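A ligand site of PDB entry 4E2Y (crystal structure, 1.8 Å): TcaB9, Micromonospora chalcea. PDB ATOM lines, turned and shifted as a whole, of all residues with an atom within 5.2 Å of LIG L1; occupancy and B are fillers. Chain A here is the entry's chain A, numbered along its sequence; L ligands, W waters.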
ATOM      1  N   ARG A  70      19.492 -16.199  20.317  1.00  0.00           N
ATOM      2  CA  ARG A  70      20.902 -15.872  20.129  1.00  0.00           C
ATOM      3  C   ARG A  70      21.884 -16.970  20.525  1.00  0.00           C
ATOM      4  O   ARG A  70      22.852 -17.237  19.802  1.00  0.00           O
ATOM      5  CB  ARG A  70      21.243 -14.496  20.699  1.00  0.00           C
ATOM      6  CG  ARG A  70      21.257 -14.470  22.268  1.00  0.00           C
ATOM      7  CD  ARG A  70      21.560 -13.048  22.712  1.00  0.00           C
ATOM      8  NE  ARG A  70      21.621 -12.954  24.176  1.00  0.00           N
ATOM      9  CZ  ARG A  70      21.894 -11.798  24.785  1.00  0.00           C
ATOM     10  NH1 ARG A  70      22.086 -10.721  24.034  1.00  0.00           N
ATOM     11  NH2 ARG A  70      21.954 -11.707  26.104  1.00  0.00           N
ATOM     12  N   PHE A  74      25.139 -18.169  18.229  1.00  0.00           N
ATOM     13  CA  PHE A  74      26.424 -17.569  18.556  1.00  0.00           C
ATOM     14  C   PHE A  74      26.955 -18.201  19.848  1.00  0.00           C
ATOM     15  O   PHE A  74      26.369 -18.005  20.920  1.00  0.00           O
ATOM     16  CB  PHE A  74      26.207 -16.050  18.678  1.00  0.00           C
ATOM     17  CG  PHE A  74      25.471 -15.480  17.482  1.00  0.00           C
ATOM     18  CD1 PHE A  74      26.068 -15.522  16.240  1.00  0.00           C
ATOM     19  CD2 PHE A  74      24.226 -14.925  17.624  1.00  0.00           C
ATOM     20  CE1 PHE A  74      25.406 -15.030  15.124  1.00  0.00           C
ATOM     21  CE2 PHE A  74      23.538 -14.427  16.538  1.00  0.00           C
ATOM     22  CZ  PHE A  74      24.149 -14.468  15.266  1.00  0.00           C
ATOM     23  N   TYR A  78      30.936 -21.485  16.382  1.00  0.00           N
ATOM     24  CA  TYR A  78      30.600 -20.681  15.225  1.00  0.00           C
ATOM     25  C   TYR A  78      31.641 -20.834  14.112  1.00  0.00           C
ATOM     26  O   TYR A  78      32.781 -20.442  14.238  1.00  0.00           O
ATOM     27  CB  TYR A  78      30.575 -19.249  15.752  1.00  0.00           C
ATOM     28  CG  TYR A  78      29.880 -18.310  14.796  1.00  0.00           C
ATOM     29  CD1 TYR A  78      30.620 -17.492  13.953  1.00  0.00           C
ATOM     30  CD2 TYR A  78      28.496 -18.225  14.781  1.00  0.00           C
ATOM     31  CE1 TYR A  78      29.990 -16.607  13.102  1.00  0.00           C
ATOM     32  CE2 TYR A  78      27.866 -17.340  13.930  1.00  0.00           C
ATOM     33  CZ  TYR A  78      28.617 -16.560  13.079  1.00  0.00           C
ATOM     34  OH  TYR A  78      27.956 -15.661  12.270  1.00  0.00           O
ATOM     35  N   TYR A  80      32.146 -19.568  11.083  1.00  0.00           N
ATOM     36  CA  TYR A  80      32.497 -18.588  10.054  1.00  0.00           C
ATOM     37  C   TYR A  80      33.640 -17.698  10.519  1.00  0.00           C
ATOM     38  O   TYR A  80      33.519 -17.001  11.521  1.00  0.00           O
ATOM     39  CB  TYR A  80      31.325 -17.645   9.765  1.00  0.00           C
ATOM     40  CG  TYR A  80      31.600 -16.733   8.592  1.00  0.00           C
ATOM     41  CD1 TYR A  80      31.499 -17.249   7.308  1.00  0.00           C
ATOM     42  CD2 TYR A  80      31.977 -15.399   8.744  1.00  0.00           C
ATOM     43  CE1 TYR A  80      31.751 -16.477   6.205  1.00  0.00           C
ATOM     44  CE2 TYR A  80      32.250 -14.588   7.641  1.00  0.00           C
ATOM     45  CZ  TYR A  80      32.092 -15.136   6.377  1.00  0.00           C
ATOM     46  OH  TYR A  80      32.313 -14.448   5.222  1.00  0.00           O
ATOM     47  N   SER A  82      35.858 -14.673   9.372  1.00  0.00           N
ATOM     48  CA  SER A  82      35.721 -13.657   8.317  1.00  0.00           C
ATOM     49  C   SER A  82      37.006 -13.594   7.506  1.00  0.00           C
ATOM     50  O   SER A  82      36.978 -13.364   6.282  1.00  0.00           O
ATOM     51  CB  SER A  82      35.494 -12.287   8.991  1.00  0.00           C
ATOM     52  OG  SER A  82      34.316 -12.344   9.780  1.00  0.00           O
ATOM     53  N   PHE A  92      38.047  -4.626   4.823  1.00  0.00           N
ATOM     54  CA  PHE A  92      38.016  -4.079   6.177  1.00  0.00           C
ATOM     55  C   PHE A  92      39.263  -3.283   6.526  1.00  0.00           C
ATOM     56  O   PHE A  92      39.163  -2.312   7.262  1.00  0.00           O
ATOM     57  CB  PHE A  92      37.717  -5.174   7.215  1.00  0.00           C
ATOM     58  CG  PHE A  92      36.317  -5.692   7.104  1.00  0.00           C
ATOM     59  CD1 PHE A  92      35.269  -4.849   7.437  1.00  0.00           C
ATOM     60  CD2 PHE A  92      36.052  -7.004   6.697  1.00  0.00           C
ATOM     61  CE1 PHE A  92      33.947  -5.284   7.350  1.00  0.00           C
ATOM     62  CE2 PHE A  92      34.727  -7.461   6.605  1.00  0.00           C
ATOM     63  CZ  PHE A  92      33.676  -6.606   6.931  1.00  0.00           C
ATOM     64  N   GLU A 113      33.950  -2.344  18.144  1.00  0.00           N
ATOM     65  CA  GLU A 113      33.317  -3.077  17.062  1.00  0.00           C
ATOM     66  C   GLU A 113      32.413  -4.165  17.668  1.00  0.00           C
ATOM     67  O   GLU A 113      32.851  -4.902  18.550  1.00  0.00           O
ATOM     68  CB  GLU A 113      34.340  -3.749  16.159  1.00  0.00           C
ATOM     69  CG  GLU A 113      33.632  -4.546  15.067  1.00  0.00           C
ATOM     70  CD  GLU A 113      34.580  -5.105  14.021  1.00  0.00           C
ATOM     71  OE1 GLU A 113      34.136  -5.328  12.871  1.00  0.00           O
ATOM     72  OE2 GLU A 113      35.775  -5.363  14.333  1.00  0.00           O
ATOM     73  N   ILE A 114      31.168  -4.164  17.182  1.00  0.00           N
ATOM     74  CA  ILE A 114      30.177  -5.204  17.475  1.00  0.00           C
ATOM     75  C   ILE A 114      30.354  -6.285  16.401  1.00  0.00           C
ATOM     76  O   ILE A 114      30.123  -6.016  15.202  1.00  0.00           O
ATOM     77  CB  ILE A 114      28.787  -4.554  17.402  1.00  0.00           C
ATOM     78  CG1 ILE A 114      28.681  -3.393  18.396  1.00  0.00           C
ATOM     79  CG2 ILE A 114      27.718  -5.637  17.577  1.00  0.00           C
ATOM     80  CD1 ILE A 114      27.382  -2.646  18.300  1.00  0.00           C
ATOM     81  N   GLY A 115      30.704  -7.474  16.855  1.00  0.00           N
ATOM     82  CA  GLY A 115      30.852  -8.677  16.019  1.00  0.00           C
ATOM     83  C   GLY A 115      32.178  -8.679  15.278  1.00  0.00           C
ATOM     84  O   GLY A 115      32.261  -8.916  14.059  1.00  0.00           O
ATOM     85  N   CYS A 116      33.228  -8.548  16.079  1.00  0.00           N
ATOM     86  CA  CYS A 116      34.544  -8.385  15.456  1.00  0.00           C
ATOM     87  C   CYS A 116      35.067  -9.688  14.849  1.00  0.00           C
ATOM     88  O   CYS A 116      36.020  -9.695  14.082  1.00  0.00           O
ATOM     89  CB  CYS A 116      35.536  -7.720  16.425  1.00  0.00           C
ATOM     90  SG  CYS A 116      35.920  -8.762  17.881  1.00  0.00           S
ATOM     91  N   ASN A 117      34.411 -10.811  15.167  1.00  0.00           N
ATOM     92  CA  ASN A 117      34.797 -12.128  14.681  1.00  0.00           C
ATOM     93  C   ASN A 117      36.302 -12.365  14.896  1.00  0.00           C
ATOM     94  O   ASN A 117      36.794 -12.061  15.985  1.00  0.00           O
ATOM     95  CB  ASN A 117      34.325 -12.208  13.202  1.00  0.00           C
ATOM     96  CG  ASN A 117      34.334 -13.605  12.641  1.00  0.00           C
ATOM     97  OD1 ASN A 117      35.314 -14.088  12.055  1.00  0.00           O
ATOM     98  ND2 ASN A 117      33.212 -14.310  12.815  1.00  0.00           N
ATOM     99  N   ILE A 120      39.228  -9.398  11.709  1.00  0.00           N
ATOM    100  CA  ILE A 120      39.388  -8.907  10.331  1.00  0.00           C
ATOM    101  C   ILE A 120      39.488  -7.385  10.188  1.00  0.00           C
ATOM    102  O   ILE A 120      40.298  -6.875   9.393  1.00  0.00           O
ATOM    103  CB  ILE A 120      38.329  -9.516   9.350  1.00  0.00           C
ATOM    104  CG1 ILE A 120      38.636  -9.175   7.886  1.00  0.00           C
ATOM    105  CG2 ILE A 120      36.913  -9.043   9.687  1.00  0.00           C
ATOM    106  CD1 ILE A 120      37.819  -9.989   6.865  1.00  0.00           C
ATOM    107  N   PHE A 135      33.448  -6.676  20.677  1.00  0.00           N
ATOM    108  CA  PHE A 135      32.490  -7.581  21.301  1.00  0.00           C
ATOM    109  C   PHE A 135      32.292  -8.776  20.370  1.00  0.00           C
ATOM    110  O   PHE A 135      31.950  -8.640  19.185  1.00  0.00           O
ATOM    111  CB  PHE A 135      31.109  -6.938  21.484  1.00  0.00           C
ATOM    112  CG  PHE A 135      31.007  -6.029  22.678  1.00  0.00           C
ATOM    113  CD1 PHE A 135      30.476  -6.492  23.873  1.00  0.00           C
ATOM    114  CD2 PHE A 135      31.519  -4.735  22.605  1.00  0.00           C
ATOM    115  CE1 PHE A 135      30.401  -5.642  24.984  1.00  0.00           C
ATOM    116  CE2 PHE A 135      31.424  -3.880  23.706  1.00  0.00           C
ATOM    117  CZ  PHE A 135      30.867  -4.331  24.911  1.00  0.00           C
ATOM    118  N   GLU A 136      32.540  -9.967  20.889  1.00  0.00           N
ATOM    119  CA  GLU A 136      32.412 -11.144  20.029  1.00  0.00           C
ATOM    120  C   GLU A 136      31.961 -12.288  20.973  1.00  0.00           C
ATOM    121  O   GLU A 136      32.796 -12.893  21.655  1.00  0.00           O
ATOM    122  CB  GLU A 136      33.729 -11.418  19.298  1.00  0.00           C
ATOM    123  CG  GLU A 136      33.708 -12.680  18.447  1.00  0.00           C
ATOM    124  CD  GLU A 136      32.414 -12.741  17.666  1.00  0.00           C
ATOM    125  OE1 GLU A 136      32.279 -11.984  16.676  1.00  0.00           O
ATOM    126  OE2 GLU A 136      31.492 -13.484  18.071  1.00  0.00           O
ATOM    127  N   PRO A 137      30.655 -12.570  20.994  1.00  0.00           N
ATOM    128  CA  PRO A 137      30.075 -13.574  21.898  1.00  0.00           C
ATOM    129  C   PRO A 137      30.466 -14.978  21.475  1.00  0.00           C
ATOM    130  O   PRO A 137      30.182 -15.910  22.211  1.00  0.00           O
ATOM    131  CB  PRO A 137      28.572 -13.367  21.728  1.00  0.00           C
ATOM    132  CG  PRO A 137      28.442 -12.826  20.290  1.00  0.00           C
ATOM    133  CD  PRO A 137      29.589 -11.836  20.274  1.00  0.00           C
ATOM    134  N   SER A 138      30.999 -15.141  20.263  1.00  0.00           N
ATOM    135  CA  SER A 138      31.345 -16.475  19.801  1.00  0.00           C
ATOM    136  C   SER A 138      32.800 -16.774  20.132  1.00  0.00           C
ATOM    137  O   SER A 138      33.741 -16.289  19.505  1.00  0.00           O
ATOM    138  CB  SER A 138      31.106 -16.672  18.312  1.00  0.00           C
ATOM    139  OG  SER A 138      29.720 -16.668  18.011  1.00  0.00           O
ATOM    140  N   VAL A 141      36.028 -17.766  17.522  1.00  0.00           N
ATOM    141  CA  VAL A 141      36.490 -16.605  16.768  1.00  0.00           C
ATOM    142  C   VAL A 141      37.039 -15.486  17.664  1.00  0.00           C
ATOM    143  O   VAL A 141      37.995 -14.805  17.299  1.00  0.00           O
ATOM    144  CB  VAL A 141      35.448 -16.067  15.738  1.00  0.00           C
ATOM    145  CG1 VAL A 141      35.108 -17.178  14.755  1.00  0.00           C
ATOM    146  CG2 VAL A 141      34.169 -15.585  16.447  1.00  0.00           C
ATOM    147  N   ASP A 155      31.233 -11.368  24.716  1.00  0.00           N
ATOM    148  CA  ASP A 155      29.926 -11.012  25.271  1.00  0.00           C
ATOM    149  C   ASP A 155      29.093 -10.523  24.111  1.00  0.00           C
ATOM    150  O   ASP A 155      29.677 -10.085  23.120  1.00  0.00           O
ATOM    151  CB  ASP A 155      29.945  -9.826  26.228  1.00  0.00           C
ATOM    152  CG  ASP A 155      30.261 -10.241  27.646  1.00  0.00           C
ATOM    153  OD1 ASP A 155      31.312  -9.781  28.141  1.00  0.00           O
ATOM    154  OD2 ASP A 155      29.461 -11.010  28.209  1.00  0.00           O
ATOM    155  N   PHE A 156      27.775 -10.571  24.276  1.00  0.00           N
ATOM    156  CA  PHE A 156      26.918  -9.875  23.326  1.00  0.00           C
ATOM    157  C   PHE A 156      26.955  -8.382  23.645  1.00  0.00           C
ATOM    158  O   PHE A 156      26.869  -7.995  24.805  1.00  0.00           O
ATOM    159  CB  PHE A 156      25.482 -10.355  23.488  1.00  0.00           C
ATOM    160  CG  PHE A 156      25.309 -11.810  23.087  1.00  0.00           C
ATOM    161  CD1 PHE A 156      25.180 -12.130  21.742  1.00  0.00           C
ATOM    162  CD2 PHE A 156      25.273 -12.837  24.044  1.00  0.00           C
ATOM    163  CE1 PHE A 156      25.017 -13.457  21.308  1.00  0.00           C
ATOM    164  CE2 PHE A 156      25.131 -14.173  23.630  1.00  0.00           C
ATOM    165  CZ  PHE A 156      24.973 -14.457  22.271  1.00  0.00           C
ATOM    166  N   PHE A 157      27.066  -7.551  22.617  1.00  0.00           N
ATOM    167  CA  PHE A 157      26.730  -6.137  22.759  1.00  0.00           C
ATOM    168  C   PHE A 157      25.223  -5.944  22.965  1.00  0.00           C
ATOM    169  O   PHE A 157      24.414  -6.420  22.185  1.00  0.00           O
ATOM    170  CB  PHE A 157      27.200  -5.336  21.534  1.00  0.00           C
ATOM    171  CG  PHE A 157      27.096  -3.840  21.730  1.00  0.00           C
ATOM    172  CD1 PHE A 157      25.912  -3.161  21.462  1.00  0.00           C
ATOM    173  CD2 PHE A 157      28.198  -3.165  22.246  1.00  0.00           C
ATOM    174  CE1 PHE A 157      25.842  -1.762  21.609  1.00  0.00           C
ATOM    175  CE2 PHE A 157      28.123  -1.763  22.424  1.00  0.00           C
ATOM    176  CZ  PHE A 157      26.955  -1.078  22.097  1.00  0.00           C
ATOM    177  N   ALA A 178      29.656  -4.747  11.202  1.00  0.00           N
ATOM    178  CA  ALA A 178      29.552  -5.214   9.826  1.00  0.00           C
ATOM    179  C   ALA A 178      28.911  -6.606   9.817  1.00  0.00           C
ATOM    180  O   ALA A 178      29.412  -7.503  10.482  1.00  0.00           O
ATOM    181  CB  ALA A 178      30.958  -5.295   9.124  1.00  0.00           C
ATOM    182  N   ASN A 179      27.847  -6.779   9.047  1.00  0.00           N
ATOM    183  CA  ASN A 179      27.244  -8.122   8.959  1.00  0.00           C
ATOM    184  C   ASN A 179      26.861  -8.642  10.346  1.00  0.00           C
ATOM    185  O   ASN A 179      26.963  -9.856  10.593  1.00  0.00           O
ATOM    186  CB  ASN A 179      28.161  -9.103   8.257  1.00  0.00           C
ATOM    187  CG  ASN A 179      28.587  -8.536   6.914  1.00  0.00           C
ATOM    188  OD1 ASN A 179      29.764  -8.248   6.670  1.00  0.00           O
ATOM    189  ND2 ASN A 179      27.614  -8.350   6.036  1.00  0.00           N
ATOM    190  N   THR A 180      26.419  -7.686  11.158  1.00  0.00           N
ATOM    191  CA  THR A 180      26.189  -8.011  12.558  1.00  0.00           C
ATOM    192  C   THR A 180      24.870  -7.431  13.040  1.00  0.00           C
ATOM    193  O   THR A 180      24.096  -8.146  13.688  1.00  0.00           O
ATOM    194  CB  THR A 180      27.381  -7.610  13.451  1.00  0.00           C
ATOM    195  OG1 THR A 180      28.538  -8.366  13.062  1.00  0.00           O
ATOM    196  CG2 THR A 180      27.070  -8.019  14.929  1.00  0.00           C
ATOM    197  N   HIS A 183      21.798  -9.231  12.319  1.00  0.00           N
ATOM    198  CA  HIS A 183      21.740 -10.568  12.928  1.00  0.00           C
ATOM    199  C   HIS A 183      21.004 -10.454  14.279  1.00  0.00           C
ATOM    200  O   HIS A 183      20.747 -11.466  14.978  1.00  0.00           O
ATOM    201  CB  HIS A 183      23.136 -11.095  13.244  1.00  0.00           C
ATOM    202  CG  HIS A 183      23.933 -11.532  12.050  1.00  0.00           C
ATOM    203  ND1 HIS A 183      23.966 -10.803  10.881  1.00  0.00           N
ATOM    204  CD2 HIS A 183      24.734 -12.594  11.835  1.00  0.00           C
ATOM    205  CE1 HIS A 183      24.728 -11.408   9.986  1.00  0.00           C
ATOM    206  NE2 HIS A 183      25.224 -12.500  10.554  1.00  0.00           N
ATOM    207  N   ILE A 184      20.699  -9.212  14.631  1.00  0.00           N
ATOM    208  CA  ILE A 184      20.279  -8.900  16.018  1.00  0.00           C
ATOM    209  C   ILE A 184      18.828  -8.383  16.137  1.00  0.00           C
ATOM    210  O   ILE A 184      18.574  -7.213  15.869  1.00  0.00           O
ATOM    211  CB  ILE A 184      21.230  -7.878  16.694  1.00  0.00           C
ATOM    212  CG1 ILE A 184      22.608  -8.494  16.949  1.00  0.00           C
ATOM    213  CG2 ILE A 184      20.733  -7.535  18.124  1.00  0.00           C
ATOM    214  CD1 ILE A 184      23.721  -7.484  17.141  1.00  0.00           C
ATOM    215  N   TYR A 186      17.113  -7.791  18.782  1.00  0.00           N
ATOM    216  CA  TYR A 186      17.078  -6.807  19.865  1.00  0.00           C
ATOM    217  C   TYR A 186      17.762  -5.473  19.596  1.00  0.00           C
ATOM    218  O   TYR A 186      18.546  -4.957  20.404  1.00  0.00           O
ATOM    219  CB  TYR A 186      17.523  -7.453  21.198  1.00  0.00           C
ATOM    220  CG  TYR A 186      18.851  -8.192  21.144  1.00  0.00           C
ATOM    221  CD1 TYR A 186      18.900  -9.491  20.629  1.00  0.00           C
ATOM    222  CD2 TYR A 186      20.039  -7.606  21.595  1.00  0.00           C
ATOM    223  CE1 TYR A 186      20.078 -10.179  20.565  1.00  0.00           C
ATOM    224  CE2 TYR A 186      21.235  -8.274  21.517  1.00  0.00           C
ATOM    225  CZ  TYR A 186      21.247  -9.553  21.003  1.00  0.00           C
ATOM    226  OH  TYR A 186      22.444 -10.225  20.996  1.00  0.00           O
ATOM    227  N   HIS A 256      29.347  -9.123  -0.451  1.00  0.00           N
ATOM    228  CA  HIS A 256      28.241  -9.934   0.061  1.00  0.00           C
ATOM    229  C   HIS A 256      26.979  -9.799  -0.746  1.00  0.00           C
ATOM    230  O   HIS A 256      25.871  -9.851  -0.187  1.00  0.00           O
ATOM    231  CB  HIS A 256      27.997  -9.737   1.547  1.00  0.00           C
ATOM    232  CG  HIS A 256      29.097 -10.313   2.387  1.00  0.00           C
ATOM    233  ND1 HIS A 256      29.444 -11.654   2.324  1.00  0.00           N
ATOM    234  CD2 HIS A 256      29.949  -9.735   3.255  1.00  0.00           C
ATOM    235  CE1 HIS A 256      30.475 -11.859   3.120  1.00  0.00           C
ATOM    236  NE2 HIS A 256      30.819 -10.716   3.689  1.00  0.00           N
HETATM  237  N1  LIG L   1      32.076  -8.485  11.297  1.00  0.00           N
HETATM  238  C1  LIG L   1      32.432  -9.807  10.736  1.00  0.00           C
HETATM  239  C2  LIG L   1      31.576 -10.936  11.306  1.00  0.00           C
HETATM  240  C3  LIG L   1      30.147 -11.049  10.781  1.00  0.00           C
HETATM  241  S1  LIG L   1      29.356 -12.487  11.449  1.00  0.00           S
HETATM  242  C4  LIG L   1      32.267  -9.744   9.239  1.00  0.00           C
HETATM  243  O1  LIG L   1      31.691  -8.754   8.785  1.00  0.00           O
HETATM  244  O2  LIG L   1      32.594 -10.651   8.481  1.00  0.00           O
HETATM  245  C5  LIG L   1      28.316 -11.870  12.750  1.00  0.00           C
HETATM  246  C6  LIG L   1      29.152 -11.872  14.030  1.00  0.00           C
HETATM  247  O3  LIG L   1      28.407 -11.203  15.054  1.00  0.00           O
HETATM  248  C7  LIG L   1      29.540 -13.229  14.634  1.00  0.00           C
HETATM  249  O4  LIG L   1      30.950 -13.381  14.913  1.00  0.00           O
HETATM  250  C8  LIG L   1      28.717 -13.256  15.917  1.00  0.00           C
HETATM  251  O5  LIG L   1      29.203 -14.099  16.973  1.00  0.00           O
HETATM  252  C9  LIG L   1      28.668 -11.797  16.325  1.00  0.00           C
HETATM  253  N2  LIG L   1      27.517 -11.390  17.180  1.00  0.00           N
HETATM  254  C10 LIG L   1      26.265 -11.891  17.257  1.00  0.00           C
HETATM  255  N3  LIG L   1      25.502 -11.148  18.102  1.00  0.00           N
HETATM  256  C11 LIG L   1      26.288 -10.182  18.641  1.00  0.00           C
HETATM  257  C12 LIG L   1      26.164  -9.050  19.597  1.00  0.00           C
HETATM  258  N4  LIG L   1      24.995  -8.851  20.239  1.00  0.00           N
HETATM  259  N5  LIG L   1      27.266  -8.291  19.855  1.00  0.00           N
HETATM  260  C13 LIG L   1      28.411  -8.503  19.187  1.00  0.00           C
HETATM  261  N6  LIG L   1      28.632  -9.489  18.292  1.00  0.00           N
HETATM  262  C14 LIG L   1      27.614 -10.343  17.998  1.00  0.00           C
HETATM  263  P1  LG2 L   2      30.203 -16.194   2.514  1.00  0.00           P
HETATM  264  C1  LG2 L   2      28.175 -15.886   6.543  1.00  0.00           C
HETATM  265  O1  LG2 L   2      27.402 -16.076   5.357  1.00  0.00           O
HETATM  266  C2  LG2 L   2      27.298 -15.965   7.790  1.00  0.00           C
HETATM  267  P2  LG2 L   2      27.959 -17.025   4.216  1.00  0.00           P
HETATM  268  C3  LG2 L   2      27.219 -14.621   8.509  1.00  0.00           C
HETATM  269  N1  LG2 L   2      25.999 -14.727   9.315  1.00  0.00           N
HETATM  270  C4  LG2 L   2      27.191 -13.468   7.523  1.00  0.00           C
HETATM  271  O2  LG2 L   2      26.364 -12.565   7.639  1.00  0.00           O
HETATM  272  C5  LG2 L   2      28.125 -13.440   6.351  1.00  0.00           C
HETATM  273  O3  LG2 L   2      28.874 -14.645   6.440  1.00  0.00           O
HETATM  274  C6  LG2 L   2      29.231 -12.387   6.429  1.00  0.00           C
HETATM  275  C7  LG2 L   2      33.726 -20.700   1.310  1.00  0.00           C
HETATM  276  N2  LG2 L   2      34.738 -20.205   0.372  1.00  0.00           N
HETATM  277  O4  LG2 L   2      31.374 -15.333   2.902  1.00  0.00           O
HETATM  278  C8  LG2 L   2      34.093 -20.255   2.720  1.00  0.00           C
HETATM  279  C9  LG2 L   2      35.494 -21.081  -0.298  1.00  0.00           C
HETATM  280  O5  LG2 L   2      35.300 -22.322  -0.211  1.00  0.00           O
HETATM  281  O6  LG2 L   2      29.478 -15.982   1.207  1.00  0.00           O
HETATM  282  C10 LG2 L   2      32.758 -20.057   3.432  1.00  0.00           C
HETATM  283  O7  LG2 L   2      32.313 -21.341   3.924  1.00  0.00           O
HETATM  284  N3  LG2 L   2      36.421 -20.644  -1.183  1.00  0.00           N
HETATM  285  C11 LG2 L   2      28.392 -14.516   9.466  1.00  0.00           C
HETATM  286  O8  LG2 L   2      26.888 -17.061   3.127  1.00  0.00           O
HETATM  287  C12 LG2 L   2      31.800 -19.758   2.283  1.00  0.00           C
HETATM  288  O9  LG2 L   2      32.471 -20.084   1.085  1.00  0.00           O
HETATM  289  C13 LG2 L   2      36.685 -19.327  -1.330  1.00  0.00           C
HETATM  290  O10 LG2 L   2      37.568 -18.892  -2.116  1.00  0.00           O
HETATM  291  O11 LG2 L   2      28.455 -18.352   4.732  1.00  0.00           O
HETATM  292  C14 LG2 L   2      31.649 -18.327   1.784  1.00  0.00           C
HETATM  293  O12 LG2 L   2      30.695 -17.713   2.606  1.00  0.00           O
HETATM  294  C15 LG2 L   2      35.853 -18.357  -0.604  1.00  0.00           C
HETATM  295  C16 LG2 L   2      36.101 -16.875  -0.746  1.00  0.00           C
HETATM  296  C17 LG2 L   2      34.904 -18.866   0.284  1.00  0.00           C
HETATM  297  O13 LG2 L   2      29.339 -16.285   3.841  1.00  0.00           O
HETATM  298  O   HOH W   1      22.963 -11.880  19.128  1.00  0.00           O
HETATM  299  O   HOH W   2      32.791 -10.648   5.732  1.00  0.00           O
HETATM  300  O   HOH W   3      34.263  -6.834  10.721  1.00  0.00           O
HETATM  301  O   HOH W   4      31.423  -6.097  12.767  1.00  0.00           O
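N of Ser 82 lies within hydrogen-bond range of OD1 of Asn 117 (2.8 Å).
The backbone carbonyl oxygen (O) of Phe 135 is in hydrogen-bond range of the backbone NH (N) of Gly 115, 2.9 Å away.
The backbone carbonyl oxygen of Asn 179 lies close to a ring nitrogen (ND1) of His 183 (3.2 Å).
The side-chain hydroxyl (OG1) of Thr 180 is in hydrogen-bond range of the backbone carbonyl oxygen (O) of Ala 178.
NH1 of Arg 70 lies within hydrogen-bond range of OH of Tyr 186, at 3.1 Å.
ND2 of Asn 117 lies within hydrogen-bond range of O of Tyr 80 (3.0 Å).
N of Phe 135 lies within hydrogen-bond range of O of Glu 113 (2.8 Å).
The backbone carbonyl oxygen (O) of Phe 135 lies within hydrogen-bond range of the backbone NH (N) of Cys 116 (3.4 Å).
Residues that only touch LIG L1: Pro 137 (3.2 Å), Ile 114 (3.4 Å), Phe 92 (3.5 Å), Phe 74 (3.5 Å), Phe 135 (3.5 Å), Phe 156 (3.6 Å), Ile 184 (3.6 Å) and His 183 (3.8 Å).
19 residues have an atom within 4 Å of LIG L1: Phe 74, Tyr 78, Ser 82, Phe 92, Ile 114, Gly 115, Asn 117, Phe 135, Glu 136, Pro 137, Ser 138, Phe 156, Phe 157, Ala 178, Asn 179, Thr 180, His 183, Ile 184 and Tyr 186.
OE2 of Glu 136 lies within hydrogen-bond range of O5 of LIG L1 (2.6 Å).
An oxygen (O2) of LIG L1 is in hydrogen-bond range of the side-chain hydroxyl of Ser 82 (2.7 Å).
A nitrogen (N6) of LIG L1 lies within hydrogen-bond range of the backbone NH (N) of Gly 115 (3.2 Å).
The backbone carbonyl oxygen (O) of Gly 115 sits at hydrogen-bond distance from a nitrogen (N1) of LIG L1, at 2.8 Å.
The side-chain hydroxyl (OG) of Ser 138 is in hydrogen-bond range of an oxygen (O5) of LIG L1 (2.8 Å).
N of Phe 157 lies within hydrogen-bond range of N5 of LIG L1 (2.9 Å).
O of Phe 157 sits at hydrogen-bond distance from N4 of LIG L1, at 3.2 Å.
OD1 of Asn 179 lies close to O1 of LIG L1 (2.9 Å).
The backbone carbonyl oxygen of Ala 178 lies within hydrogen-bond range of a nitrogen (N1) of LIG L1, at 3.0 Å.
A nitrogen (N4) of LIG L1 sits at hydrogen-bond distance from the side-chain hydroxyl (OH) of Tyr 186 (3.0 Å).
The side-chain amide nitrogen (ND2) of Asn 117 sits at hydrogen-bond distance from an oxygen (O4) of LIG L1 (3.2 Å).
The side-chain hydroxyl (OG1) of Thr 180 lies close to an oxygen (O3) of LIG L1, 3.5 Å away.
The side-chain hydroxyl (OH) of Tyr 78 lies close to a sulfur (S1) of LIG L1 (3.6 Å).
A ring nitrogen (NE2) of His 183 is in hydrogen-bond range of a nitrogen (N1) of LG2 L2, at 2.7 Å.
An oxygen (O4) of LG2 L2 is in hydrogen-bond range of the side-chain hydroxyl of Tyr 80.
Water W2 lies within hydrogen-bond range of an oxygen (O2) of LIG L1 (2.8 Å) and a ring nitrogen (NE2) of His 256 (2.8 Å).
Water W3 lies within hydrogen-bond range of the side-chain carboxylate of Glu 113 (2.6 Å) and a nitrogen (N1) of LIG L1 (2.8 Å).
Water W1 bridges OH of Tyr 186 and N3 of LIG L1.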
